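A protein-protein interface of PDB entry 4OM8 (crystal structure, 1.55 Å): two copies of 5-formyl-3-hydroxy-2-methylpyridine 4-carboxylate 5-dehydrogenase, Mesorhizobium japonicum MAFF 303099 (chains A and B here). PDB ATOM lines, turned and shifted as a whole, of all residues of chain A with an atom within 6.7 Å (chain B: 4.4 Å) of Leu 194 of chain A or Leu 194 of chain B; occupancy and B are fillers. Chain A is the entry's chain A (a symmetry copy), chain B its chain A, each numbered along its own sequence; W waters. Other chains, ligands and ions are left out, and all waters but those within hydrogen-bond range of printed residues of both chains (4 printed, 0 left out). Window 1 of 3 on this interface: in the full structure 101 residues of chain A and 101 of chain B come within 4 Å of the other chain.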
ATOM      1  N   ARG A 189     -18.951 -27.294  18.418  1.00  0.00           N
ATOM      2  CA  ARG A 189     -18.109 -26.158  18.805  1.00  0.00           C
ATOM      3  C   ARG A 189     -17.654 -26.297  20.247  1.00  0.00           C
ATOM      4  O   ARG A 189     -16.469 -26.138  20.568  1.00  0.00           O
ATOM      5  CB  ARG A 189     -18.845 -24.829  18.639  1.00  0.00           C
ATOM      6  CG  ARG A 189     -19.065 -24.442  17.191  1.00  0.00           C
ATOM      7  CD  ARG A 189     -19.593 -23.019  17.068  1.00  0.00           C
ATOM      8  NE  ARG A 189     -18.633 -21.980  17.409  1.00  0.00           N
ATOM      9  CZ  ARG A 189     -17.807 -21.411  16.538  1.00  0.00           C
ATOM     10  NH1 ARG A 189     -17.809 -21.772  15.263  1.00  0.00           N
ATOM     11  NH2 ARG A 189     -16.979 -20.457  16.953  1.00  0.00           N
ATOM     12  N   VAL A 190     -18.598 -26.601  21.128  1.00  0.00           N
ATOM     13  CA  VAL A 190     -18.242 -26.728  22.525  1.00  0.00           C
ATOM     14  C   VAL A 190     -17.344 -27.962  22.713  1.00  0.00           C
ATOM     15  O   VAL A 190     -16.357 -27.915  23.456  1.00  0.00           O
ATOM     16  CB  VAL A 190     -19.493 -26.792  23.420  1.00  0.00           C
ATOM     17  CG1 VAL A 190     -19.103 -26.999  24.875  1.00  0.00           C
ATOM     18  CG2 VAL A 190     -20.303 -25.502  23.283  1.00  0.00           C
ATOM     19  N   LEU A 191     -17.640 -29.045  21.998  1.00  0.00           N
ATOM     20  CA  LEU A 191     -16.795 -30.234  22.084  1.00  0.00           C
ATOM     21  C   LEU A 191     -15.375 -29.959  21.598  1.00  0.00           C
ATOM     22  O   LEU A 191     -14.395 -30.346  22.243  1.00  0.00           O
ATOM     23  CB  LEU A 191     -17.392 -31.381  21.262  1.00  0.00           C
ATOM     24  CG  LEU A 191     -16.543 -32.662  21.241  1.00  0.00           C
ATOM     25  CD1 LEU A 191     -16.363 -33.258  22.642  1.00  0.00           C
ATOM     26  CD2 LEU A 191     -17.132 -33.691  20.276  1.00  0.00           C
ATOM     27  N   TYR A 192     -15.259 -29.289  20.456  1.00  0.00           N
ATOM     28  CA  TYR A 192     -13.933 -29.034  19.913  1.00  0.00           C
ATOM     29  C   TYR A 192     -13.180 -28.008  20.761  1.00  0.00           C
ATOM     30  O   TYR A 192     -11.959 -28.031  20.797  1.00  0.00           O
ATOM     31  CB  TYR A 192     -14.015 -28.613  18.429  1.00  0.00           C
ATOM     32  CG  TYR A 192     -13.970 -29.830  17.518  1.00  0.00           C
ATOM     33  CD1 TYR A 192     -14.977 -30.784  17.540  1.00  0.00           C
ATOM     34  CD2 TYR A 192     -12.895 -30.044  16.669  1.00  0.00           C
ATOM     35  CE1 TYR A 192     -14.913 -31.917  16.723  1.00  0.00           C
ATOM     36  CE2 TYR A 192     -12.820 -31.156  15.861  1.00  0.00           C
ATOM     37  CZ  TYR A 192     -13.823 -32.087  15.885  1.00  0.00           C
ATOM     38  OH  TYR A 192     -13.710 -33.183  15.056  1.00  0.00           O
ATOM     39  N   ALA A 193     -13.881 -27.146  21.488  1.00  0.00           N
ATOM     40  CA  ALA A 193     -13.179 -26.264  22.420  1.00  0.00           C
ATOM     41  C   ALA A 193     -12.583 -27.063  23.580  1.00  0.00           C
ATOM     42  O   ALA A 193     -11.441 -26.838  23.982  1.00  0.00           O
ATOM     43  CB  ALA A 193     -14.114 -25.186  22.935  1.00  0.00           C
ATOM     44  N   LEU A 194     -13.368 -27.997  24.116  1.00  0.00           N
ATOM     45  CA  LEU A 194     -12.892 -28.918  25.151  1.00  0.00           C
ATOM     46  C   LEU A 194     -11.686 -29.697  24.639  1.00  0.00           C
ATOM     47  O   LEU A 194     -10.647 -29.757  25.301  1.00  0.00           O
ATOM     48  CB  LEU A 194     -14.026 -29.868  25.568  1.00  0.00           C
ATOM     49  CG  LEU A 194     -13.872 -30.948  26.640  1.00  0.00           C
ATOM     50  CD1 LEU A 194     -15.271 -31.372  27.068  1.00  0.00           C
ATOM     51  CD2 LEU A 194     -13.112 -32.160  26.127  1.00  0.00           C
ATOM     52  N   LEU A 195     -11.828 -30.287  23.453  1.00  0.00           N
ATOM     53  CA  LEU A 195     -10.774 -31.116  22.872  1.00  0.00           C
ATOM     54  C   LEU A 195      -9.515 -30.319  22.575  1.00  0.00           C
ATOM     55  O   LEU A 195      -8.411 -30.818  22.775  1.00  0.00           O
ATOM     56  CB  LEU A 195     -11.269 -31.783  21.582  1.00  0.00           C
ATOM     57  CG  LEU A 195     -12.330 -32.866  21.795  1.00  0.00           C
ATOM     58  CD1 LEU A 195     -12.862 -33.345  20.461  1.00  0.00           C
ATOM     59  CD2 LEU A 195     -11.749 -34.046  22.580  1.00  0.00           C
ATOM     60  N   ARG A 196      -9.672 -29.085  22.096  1.00  0.00           N
ATOM     61  CA  ARG A 196      -8.496 -28.280  21.775  1.00  0.00           C
ATOM     62  C   ARG A 196      -7.599 -28.111  23.005  1.00  0.00           C
ATOM     63  O   ARG A 196      -6.371 -28.273  22.930  1.00  0.00           O
ATOM     64  CB  ARG A 196      -8.911 -26.915  21.223  1.00  0.00           C
ATOM     65  CG  ARG A 196      -7.713 -26.017  20.866  1.00  0.00           C
ATOM     66  CD  ARG A 196      -8.158 -24.782  20.123  1.00  0.00           C
ATOM     67  NE  ARG A 196      -9.046 -23.940  20.911  1.00  0.00           N
ATOM     68  CZ  ARG A 196      -9.328 -22.676  20.608  1.00  0.00           C
ATOM     69  NH1 ARG A 196      -8.765 -22.121  19.538  1.00  0.00           N
ATOM     70  NH2 ARG A 196     -10.154 -21.963  21.378  1.00  0.00           N
ATOM     71  N   GLU A 197      -8.214 -27.840  24.150  1.00  0.00           N
ATOM     72  CA  GLU A 197      -7.430 -27.669  25.381  1.00  0.00           C
ATOM     73  C   GLU A 197      -6.889 -29.005  25.892  1.00  0.00           C
ATOM     74  O   GLU A 197      -5.729 -29.097  26.297  1.00  0.00           O
ATOM     75  CB  GLU A 197      -8.277 -26.984  26.461  1.00  0.00           C
ATOM     76  CG  GLU A 197      -7.513 -26.648  27.744  1.00  0.00           C
ATOM     77  CD  GLU A 197      -6.380 -25.666  27.531  1.00  0.00           C
ATOM     78  OE1 GLU A 197      -5.376 -25.762  28.261  1.00  0.00           O
ATOM     79  OE2 GLU A 197      -6.470 -24.789  26.642  1.00  0.00           O
ATOM     80  N   ALA A 198      -7.724 -30.046  25.850  1.00  0.00           N
ATOM     81  CA  ALA A 198      -7.285 -31.360  26.319  1.00  0.00           C
ATOM     82  C   ALA A 198      -6.101 -31.869  25.500  1.00  0.00           C
ATOM     83  O   ALA A 198      -5.119 -32.357  26.056  1.00  0.00           O
ATOM     84  CB  ALA A 198      -8.433 -32.357  26.266  1.00  0.00           C
ATOM     85  N   VAL A 199      -6.195 -31.743  24.182  1.00  0.00           N
ATOM     86  CA  VAL A 199      -5.113 -32.184  23.312  1.00  0.00           C
ATOM     87  C   VAL A 199      -3.845 -31.368  23.607  1.00  0.00           C
ATOM     88  O   VAL A 199      -2.750 -31.922  23.674  1.00  0.00           O
ATOM     89  CB  VAL A 199      -5.515 -32.061  21.835  1.00  0.00           C
ATOM     90  CG1 VAL A 199      -4.278 -32.136  20.907  1.00  0.00           C
ATOM     91  CG2 VAL A 199      -6.540 -33.150  21.490  1.00  0.00           C
ATOM     92  N   LEU A 212      -5.649 -37.740  31.609  1.00  0.00           N
ATOM     93  CA  LEU A 212      -6.515 -36.706  31.058  1.00  0.00           C
ATOM     94  C   LEU A 212      -7.960 -37.224  31.034  1.00  0.00           C
ATOM     95  O   LEU A 212      -8.893 -36.545  31.472  1.00  0.00           O
ATOM     96  CB  LEU A 212      -6.047 -36.321  29.641  1.00  0.00           C
ATOM     97  CG  LEU A 212      -6.753 -35.218  28.839  1.00  0.00           C
ATOM     98  CD1 LEU A 212      -8.141 -35.621  28.303  1.00  0.00           C
ATOM     99  CD2 LEU A 212      -6.823 -33.924  29.633  1.00  0.00           C
ATOM    100  N   VAL A 216     -11.080 -35.641  33.037  1.00  0.00           N
ATOM    101  CA  VAL A 216     -12.185 -34.967  32.367  1.00  0.00           C
ATOM    102  C   VAL A 216     -13.497 -35.767  32.445  1.00  0.00           C
ATOM    103  O   VAL A 216     -14.559 -35.188  32.654  1.00  0.00           O
ATOM    104  CB  VAL A 216     -11.812 -34.649  30.898  1.00  0.00           C
ATOM    105  CG1 VAL A 216     -13.003 -34.052  30.159  1.00  0.00           C
ATOM    106  CG2 VAL A 216     -10.606 -33.687  30.846  1.00  0.00           C
ATOM    107  N   ILE A 220     -15.520 -33.394  34.812  1.00  0.00           N
ATOM    108  CA  ILE A 220     -16.265 -32.524  33.902  1.00  0.00           C
ATOM    109  C   ILE A 220     -17.468 -33.242  33.278  1.00  0.00           C
ATOM    110  O   ILE A 220     -18.595 -32.820  33.472  1.00  0.00           O
ATOM    111  CB  ILE A 220     -15.349 -31.960  32.783  1.00  0.00           C
ATOM    112  CG1 ILE A 220     -14.236 -31.134  33.420  1.00  0.00           C
ATOM    113  CG2 ILE A 220     -16.151 -31.074  31.831  1.00  0.00           C
ATOM    114  CD1 ILE A 220     -13.171 -30.671  32.459  1.00  0.00           C
ATOM    115  N   GLY A 221     -17.249 -34.313  32.521  1.00  0.00           N
ATOM    116  CA  GLY A 221     -18.372 -34.951  31.829  1.00  0.00           C
ATOM    117  C   GLY A 221     -19.456 -35.453  32.783  1.00  0.00           C
ATOM    118  O   GLY A 221     -20.645 -35.208  32.590  1.00  0.00           O
ATOM    119  N   ILE A 224     -21.309 -32.405  34.153  1.00  0.00           N
ATOM    120  CA  ILE A 224     -22.066 -31.678  33.120  1.00  0.00           C
ATOM    121  C   ILE A 224     -23.244 -32.496  32.583  1.00  0.00           C
ATOM    122  O   ILE A 224     -24.260 -31.935  32.145  1.00  0.00           O
ATOM    123  CB  ILE A 224     -21.130 -31.250  31.961  1.00  0.00           C
ATOM    124  CG1 ILE A 224     -20.154 -30.166  32.438  1.00  0.00           C
ATOM    125  CG2 ILE A 224     -21.919 -30.762  30.749  1.00  0.00           C
ATOM    126  CD1 ILE A 224     -20.761 -28.796  32.534  1.00  0.00           C
ATOM    127  N   PRO A 229     -23.699 -26.464  31.488  1.00  0.00           N
ATOM    128  CA  PRO A 229     -22.742 -25.379  31.762  1.00  0.00           C
ATOM    129  C   PRO A 229     -23.348 -24.078  32.320  1.00  0.00           C
ATOM    130  O   PRO A 229     -22.731 -23.484  33.205  1.00  0.00           O
ATOM    131  CB  PRO A 229     -22.113 -25.106  30.387  1.00  0.00           C
ATOM    132  CG  PRO A 229     -22.329 -26.347  29.589  1.00  0.00           C
ATOM    133  CD  PRO A 229     -23.591 -26.986  30.110  1.00  0.00           C
ATOM    134  N   TYR A 241     -16.833 -17.214  38.502  1.00  0.00           N
ATOM    135  CA  TYR A 241     -16.492 -17.373  37.091  1.00  0.00           C
ATOM    136  C   TYR A 241     -15.853 -16.101  36.536  1.00  0.00           C
ATOM    137  O   TYR A 241     -14.896 -16.179  35.783  1.00  0.00           O
ATOM    138  CB  TYR A 241     -17.717 -17.753  36.263  1.00  0.00           C
ATOM    139  CG  TYR A 241     -17.365 -18.033  34.818  1.00  0.00           C
ATOM    140  CD1 TYR A 241     -16.471 -19.056  34.479  1.00  0.00           C
ATOM    141  CD2 TYR A 241     -17.899 -17.265  33.795  1.00  0.00           C
ATOM    142  CE1 TYR A 241     -16.137 -19.305  33.145  1.00  0.00           C
ATOM    143  CE2 TYR A 241     -17.568 -17.495  32.467  1.00  0.00           C
ATOM    144  CZ  TYR A 241     -16.697 -18.516  32.149  1.00  0.00           C
ATOM    145  OH  TYR A 241     -16.379 -18.719  30.823  1.00  0.00           O
ATOM    146  N   LEU A 252      -5.568 -19.940  28.251  1.00  0.00           N
ATOM    147  CA  LEU A 252      -6.015 -21.118  27.501  1.00  0.00           C
ATOM    148  C   LEU A 252      -5.376 -21.211  26.112  1.00  0.00           C
ATOM    149  O   LEU A 252      -4.995 -20.193  25.525  1.00  0.00           O
ATOM    150  CB  LEU A 252      -7.532 -21.086  27.353  1.00  0.00           C
ATOM    151  CG  LEU A 252      -8.314 -21.216  28.659  1.00  0.00           C
ATOM    152  CD1 LEU A 252      -9.802 -21.079  28.378  1.00  0.00           C
ATOM    153  CD2 LEU A 252      -7.993 -22.547  29.345  1.00  0.00           C
ATOM    154  N   VAL B 190      -9.659 -27.471  31.163  1.00  0.00           N
ATOM    155  CA  VAL B 190     -10.538 -28.051  30.170  1.00  0.00           C
ATOM    156  C   VAL B 190     -11.971 -27.543  30.396  1.00  0.00           C
ATOM    157  O   VAL B 190     -12.681 -27.214  29.438  1.00  0.00           O
ATOM    158  CB  VAL B 190     -10.469 -29.589  30.189  1.00  0.00           C
ATOM    159  CG1 VAL B 190     -11.450 -30.183  29.192  1.00  0.00           C
ATOM    160  CG2 VAL B 190      -9.052 -30.056  29.857  1.00  0.00           C
ATOM    161  N   LEU B 191     -12.380 -27.414  31.657  1.00  0.00           N
ATOM    162  CA  LEU B 191     -13.709 -26.882  31.946  1.00  0.00           C
ATOM    163  C   LEU B 191     -13.867 -25.446  31.454  1.00  0.00           C
ATOM    164  O   LEU B 191     -14.872 -25.092  30.829  1.00  0.00           O
ATOM    165  CB  LEU B 191     -13.995 -26.931  33.450  1.00  0.00           C
ATOM    166  CG  LEU B 191     -15.351 -26.336  33.863  1.00  0.00           C
ATOM    167  CD1 LEU B 191     -16.528 -27.090  33.233  1.00  0.00           C
ATOM    168  CD2 LEU B 191     -15.482 -26.282  35.385  1.00  0.00           C
ATOM    169  N   TYR B 192     -12.871 -24.610  31.737  1.00  0.00           N
ATOM    170  CA  TYR B 192     -12.979 -23.216  31.338  1.00  0.00           C
ATOM    171  C   TYR B 192     -12.866 -23.068  29.820  1.00  0.00           C
ATOM    172  O   TYR B 192     -13.409 -22.128  29.260  1.00  0.00           O
ATOM    173  CB  TYR B 192     -11.944 -22.345  32.085  1.00  0.00           C
ATOM    174  CG  TYR B 192     -12.512 -21.838  33.400  1.00  0.00           C
ATOM    175  CD1 TYR B 192     -12.855 -22.712  34.422  1.00  0.00           C
ATOM    176  CD2 TYR B 192     -12.748 -20.486  33.600  1.00  0.00           C
ATOM    177  CE1 TYR B 192     -13.407 -22.241  35.617  1.00  0.00           C
ATOM    178  CE2 TYR B 192     -13.293 -20.010  34.771  1.00  0.00           C
ATOM    179  CZ  TYR B 192     -13.619 -20.881  35.775  1.00  0.00           C
ATOM    180  OH  TYR B 192     -14.158 -20.361  36.934  1.00  0.00           O
ATOM    181  N   ALA B 193     -12.220 -24.006  29.136  1.00  0.00           N
ATOM    182  CA  ALA B 193     -12.237 -23.960  27.674  1.00  0.00           C
ATOM    183  C   ALA B 193     -13.639 -24.252  27.138  1.00  0.00           C
ATOM    184  O   ALA B 193     -14.119 -23.581  26.224  1.00  0.00           O
ATOM    185  CB  ALA B 193     -11.229 -24.938  27.102  1.00  0.00           C
ATOM    186  N   LEU B 194     -14.290 -25.263  27.712  1.00  0.00           N
ATOM    187  CA  LEU B 194     -15.681 -25.582  27.385  1.00  0.00           C
ATOM    188  C   LEU B 194     -16.569 -24.372  27.651  1.00  0.00           C
ATOM    189  O   LEU B 194     -17.349 -23.961  26.788  1.00  0.00           O
ATOM    190  CB  LEU B 194     -16.146 -26.798  28.204  1.00  0.00           C
ATOM    191  CG  LEU B 194     -17.546 -27.405  28.095  1.00  0.00           C
ATOM    192  CD1 LEU B 194     -17.489 -28.799  28.705  1.00  0.00           C
ATOM    193  CD2 LEU B 194     -18.589 -26.575  28.827  1.00  0.00           C
ATOM    194  N   LEU B 195     -16.441 -23.801  28.848  1.00  0.00           N
ATOM    195  CA  LEU B 195     -17.274 -22.672  29.257  1.00  0.00           C
ATOM    196  C   LEU B 195     -17.036 -21.442  28.397  1.00  0.00           C
ATOM    197  O   LEU B 195     -17.981 -20.727  28.073  1.00  0.00           O
ATOM    198  CB  LEU B 195     -17.012 -22.321  30.727  1.00  0.00           C
ATOM    199  CG  LEU B 195     -17.520 -23.363  31.727  1.00  0.00           C
ATOM    200  CD1 LEU B 195     -17.075 -23.002  33.129  1.00  0.00           C
ATOM    201  CD2 LEU B 195     -19.047 -23.465  31.675  1.00  0.00           C
ATOM    202  N   ARG B 196     -15.781 -21.188  28.027  1.00  0.00           N
ATOM    203  CA  ARG B 196     -15.492 -20.009  27.214  1.00  0.00           C
ATOM    204  C   ARG B 196     -16.287 -20.040  25.906  1.00  0.00           C
ATOM    205  O   ARG B 196     -16.894 -19.037  25.500  1.00  0.00           O
ATOM    206  CB  ARG B 196     -13.993 -19.906  26.929  1.00  0.00           C
ATOM    207  CG  ARG B 196     -13.624 -18.681  26.073  1.00  0.00           C
ATOM    208  CD  ARG B 196     -12.128 -18.493  26.004  1.00  0.00           C
ATOM    209  NE  ARG B 196     -11.449 -19.617  25.377  1.00  0.00           N
ATOM    210  CZ  ARG B 196     -10.197 -19.567  24.929  1.00  0.00           C
ATOM    211  NH1 ARG B 196      -9.512 -18.432  25.035  1.00  0.00           N
ATOM    212  NH2 ARG B 196      -9.636 -20.640  24.365  1.00  0.00           N
ATOM    213  N   GLU B 197     -16.333 -21.206  25.272  1.00  0.00           N
ATOM    214  CA  GLU B 197     -17.080 -21.326  24.012  1.00  0.00           C
ATOM    215  C   GLU B 197     -18.590 -21.303  24.251  1.00  0.00           C
ATOM    216  O   GLU B 197     -19.329 -20.641  23.520  1.00  0.00           O
ATOM    217  CB  GLU B 197     -16.672 -22.606  23.271  1.00  0.00           C
ATOM    218  CG  GLU B 197     -17.304 -22.763  21.887  1.00  0.00           C
ATOM    219  CD  GLU B 197     -16.905 -21.672  20.915  1.00  0.00           C
ATOM    220  OE1 GLU B 197     -17.730 -21.332  20.046  1.00  0.00           O
ATOM    221  OE2 GLU B 197     -15.776 -21.140  21.000  1.00  0.00           O
ATOM    222  N   ALA B 198     -19.044 -22.008  25.289  1.00  0.00           N
ATOM    223  CA  ALA B 198     -20.475 -22.040  25.588  1.00  0.00           C
ATOM    224  C   ALA B 198     -21.003 -20.640  25.898  1.00  0.00           C
ATOM    225  O   ALA B 198     -22.048 -20.238  25.392  1.00  0.00           O
ATOM    226  CB  ALA B 198     -20.759 -22.981  26.748  1.00  0.00           C
ATOM    227  N   ILE B 220     -22.470 -33.861  25.006  1.00  0.00           N
ATOM    228  CA  ILE B 220     -21.063 -33.834  25.404  1.00  0.00           C
ATOM    229  C   ILE B 220     -20.846 -34.452  26.791  1.00  0.00           C
ATOM    230  O   ILE B 220     -20.130 -35.430  26.914  1.00  0.00           O
ATOM    231  CB  ILE B 220     -20.496 -32.389  25.376  1.00  0.00           C
ATOM    232  CG1 ILE B 220     -20.596 -31.842  23.955  1.00  0.00           C
ATOM    233  CG2 ILE B 220     -19.033 -32.380  25.817  1.00  0.00           C
ATOM    234  CD1 ILE B 220     -20.242 -30.384  23.819  1.00  0.00           C
ATOM    235  N   PRO B 229     -12.091 -37.810  26.628  1.00  0.00           N
ATOM    236  CA  PRO B 229     -11.757 -37.147  25.356  1.00  0.00           C
ATOM    237  C   PRO B 229     -10.729 -37.876  24.471  1.00  0.00           C
ATOM    238  O   PRO B 229     -10.916 -37.888  23.254  1.00  0.00           O
ATOM    239  CB  PRO B 229     -11.184 -35.793  25.802  1.00  0.00           C
ATOM    240  CG  PRO B 229     -11.714 -35.561  27.176  1.00  0.00           C
ATOM    241  CD  PRO B 229     -11.926 -36.920  27.796  1.00  0.00           C
HETATM  242  O   HOH W   1     -18.234 -18.861  19.363  1.00  0.00           O
HETATM  243  O   HOH W   2      -8.407 -23.693  25.027  1.00  0.00           O
HETATM  244  O   HOH W   3     -13.375 -21.608  22.256  1.00  0.00           O
HETATM  245  O   HOH W   4     -13.956 -19.722  30.518  1.00  0.00           O
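OE1 of Glu 197 of chain B is in salt-bridge range of NE of Arg 189 of chain A. The guanidinium group (NH2) of Arg 196 of chain B lies close to the guanidinium group (NH2) of Arg 196 of chain A.
The backbone carbonyl oxygen (O) of Val 216 of chain A lies within hydrogen-bond range of the backbone NH (N) of Gly 221 of chain A (2.8 Å).
N of Leu 191 of chain A touches CD1 of Ile 220 of chain B (3.4 Å). Glu 197 of chain B touches Ala 193 of chain A. CD2 of Leu 194 of chain A touches CG of Pro 229 of chain B, 3.8 Å away. CB of Ala 193 of chain B touches CB of Glu 197 of chain A, 3.6 Å away. CD1 of Leu 212 of chain A touches CG of Pro 229 of chain B, 3.7 Å away. CG of Pro 229 of chain A touches CD2 of Leu 194 of chain B, 3.8 Å away. Leu 195 of chain B touches Pro 229 of chain A. Tyr 192 of chain B touches Tyr 241 of chain A. N of Arg 196 of chain B touches OH of Tyr 241 of chain A (3.8 Å). CB of Leu 252 of chain A touches NH2 of Arg 196 of chain B, at 3.7 Å.
Of chain B, only Val 190 (3.6 Å), Leu 194 (3.8 Å) and Pro 229 (3.8 Å) come within 4 Å of Leu 194 of chain A. Printed residues of chain B within 4 Å of Leu 195 of chain A: Pro 229. Val 199 of chain A touches none of the printed residues of chain B. Printed residues of chain B within 4 Å of Tyr 241 of chain A: Tyr 192, Leu 195 and Arg 196. Printed residues of chain A within 4 Å of Tyr 192 of chain B: Tyr 241 and Leu 252. Of the printed residues of chain A, Pro 229 of chain B touches Leu 194 (3.8 Å), Leu 195 (3.7 Å), Leu 212 (3.7 Å) and Val 216 (3.6 Å). The nearest residue of chain A that does not touch Leu 194 of chain B is Ile 220 of chain A (4.1 Å).
Of the 19 printed residues of chain A, 14 touch a printed residue of chain B. Hydrophobic or aromatic side chains of chain B within 4 Å of the printed part of chain A: Val 190, Leu 191, Tyr 192, Ala 193, Leu 194, Leu 195, Ile 220 and Pro 229. Among the printed residues, Asp or Glu carboxylates within 4 Å of a Lys or Arg side-chain nitrogen of the other chain: Arg 189 of chain A with Glu 197 of chain B (2.9 Å).
Val 190 of chain A touches Leu 194 of chain B, and with the chains exchanged Leu 194 of chain A touches Val 190 of chain B. Ala 193 of chain B touches its own counterpart, Ala 193 of chain A. Ala 193 of chain A touches Glu 197 of chain B, and with the chains exchanged Glu 197 of chain A touches Ala 193 of chain B. Leu 195 of chain A touches Pro 229 of chain B, and with the chains exchanged Pro 229 of chain A touches Leu 195 of chain B. Positions printed for both chains: 190, 191, 192, 193, 194, 195, 196, 197, 198, 220 and 229. Of the 25 pairs that touch across the chains among the printed residues, 15 have their exchanged pair printed and touching as well.
Water W1 bridges OE1 of Glu 197 of chain B (2.6 Å) and NH2 of Arg 189 of chain A (3.2 Å). Water W4 lies within hydrogen-bond range of OH of Tyr 241 of chain A, O of Tyr 192 of chain B and N of Arg 196 of chain B. Water W3 bridges the side-chain carboxylate (OE2) of Glu 197 of chain B (2.7 Å) and the guanidinium group (NH2) of Arg 196 of chain A (3.4 Å). Water W2 bridges OE2 of Glu 197 of chain A and NH2 of Arg 196 of chain B.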
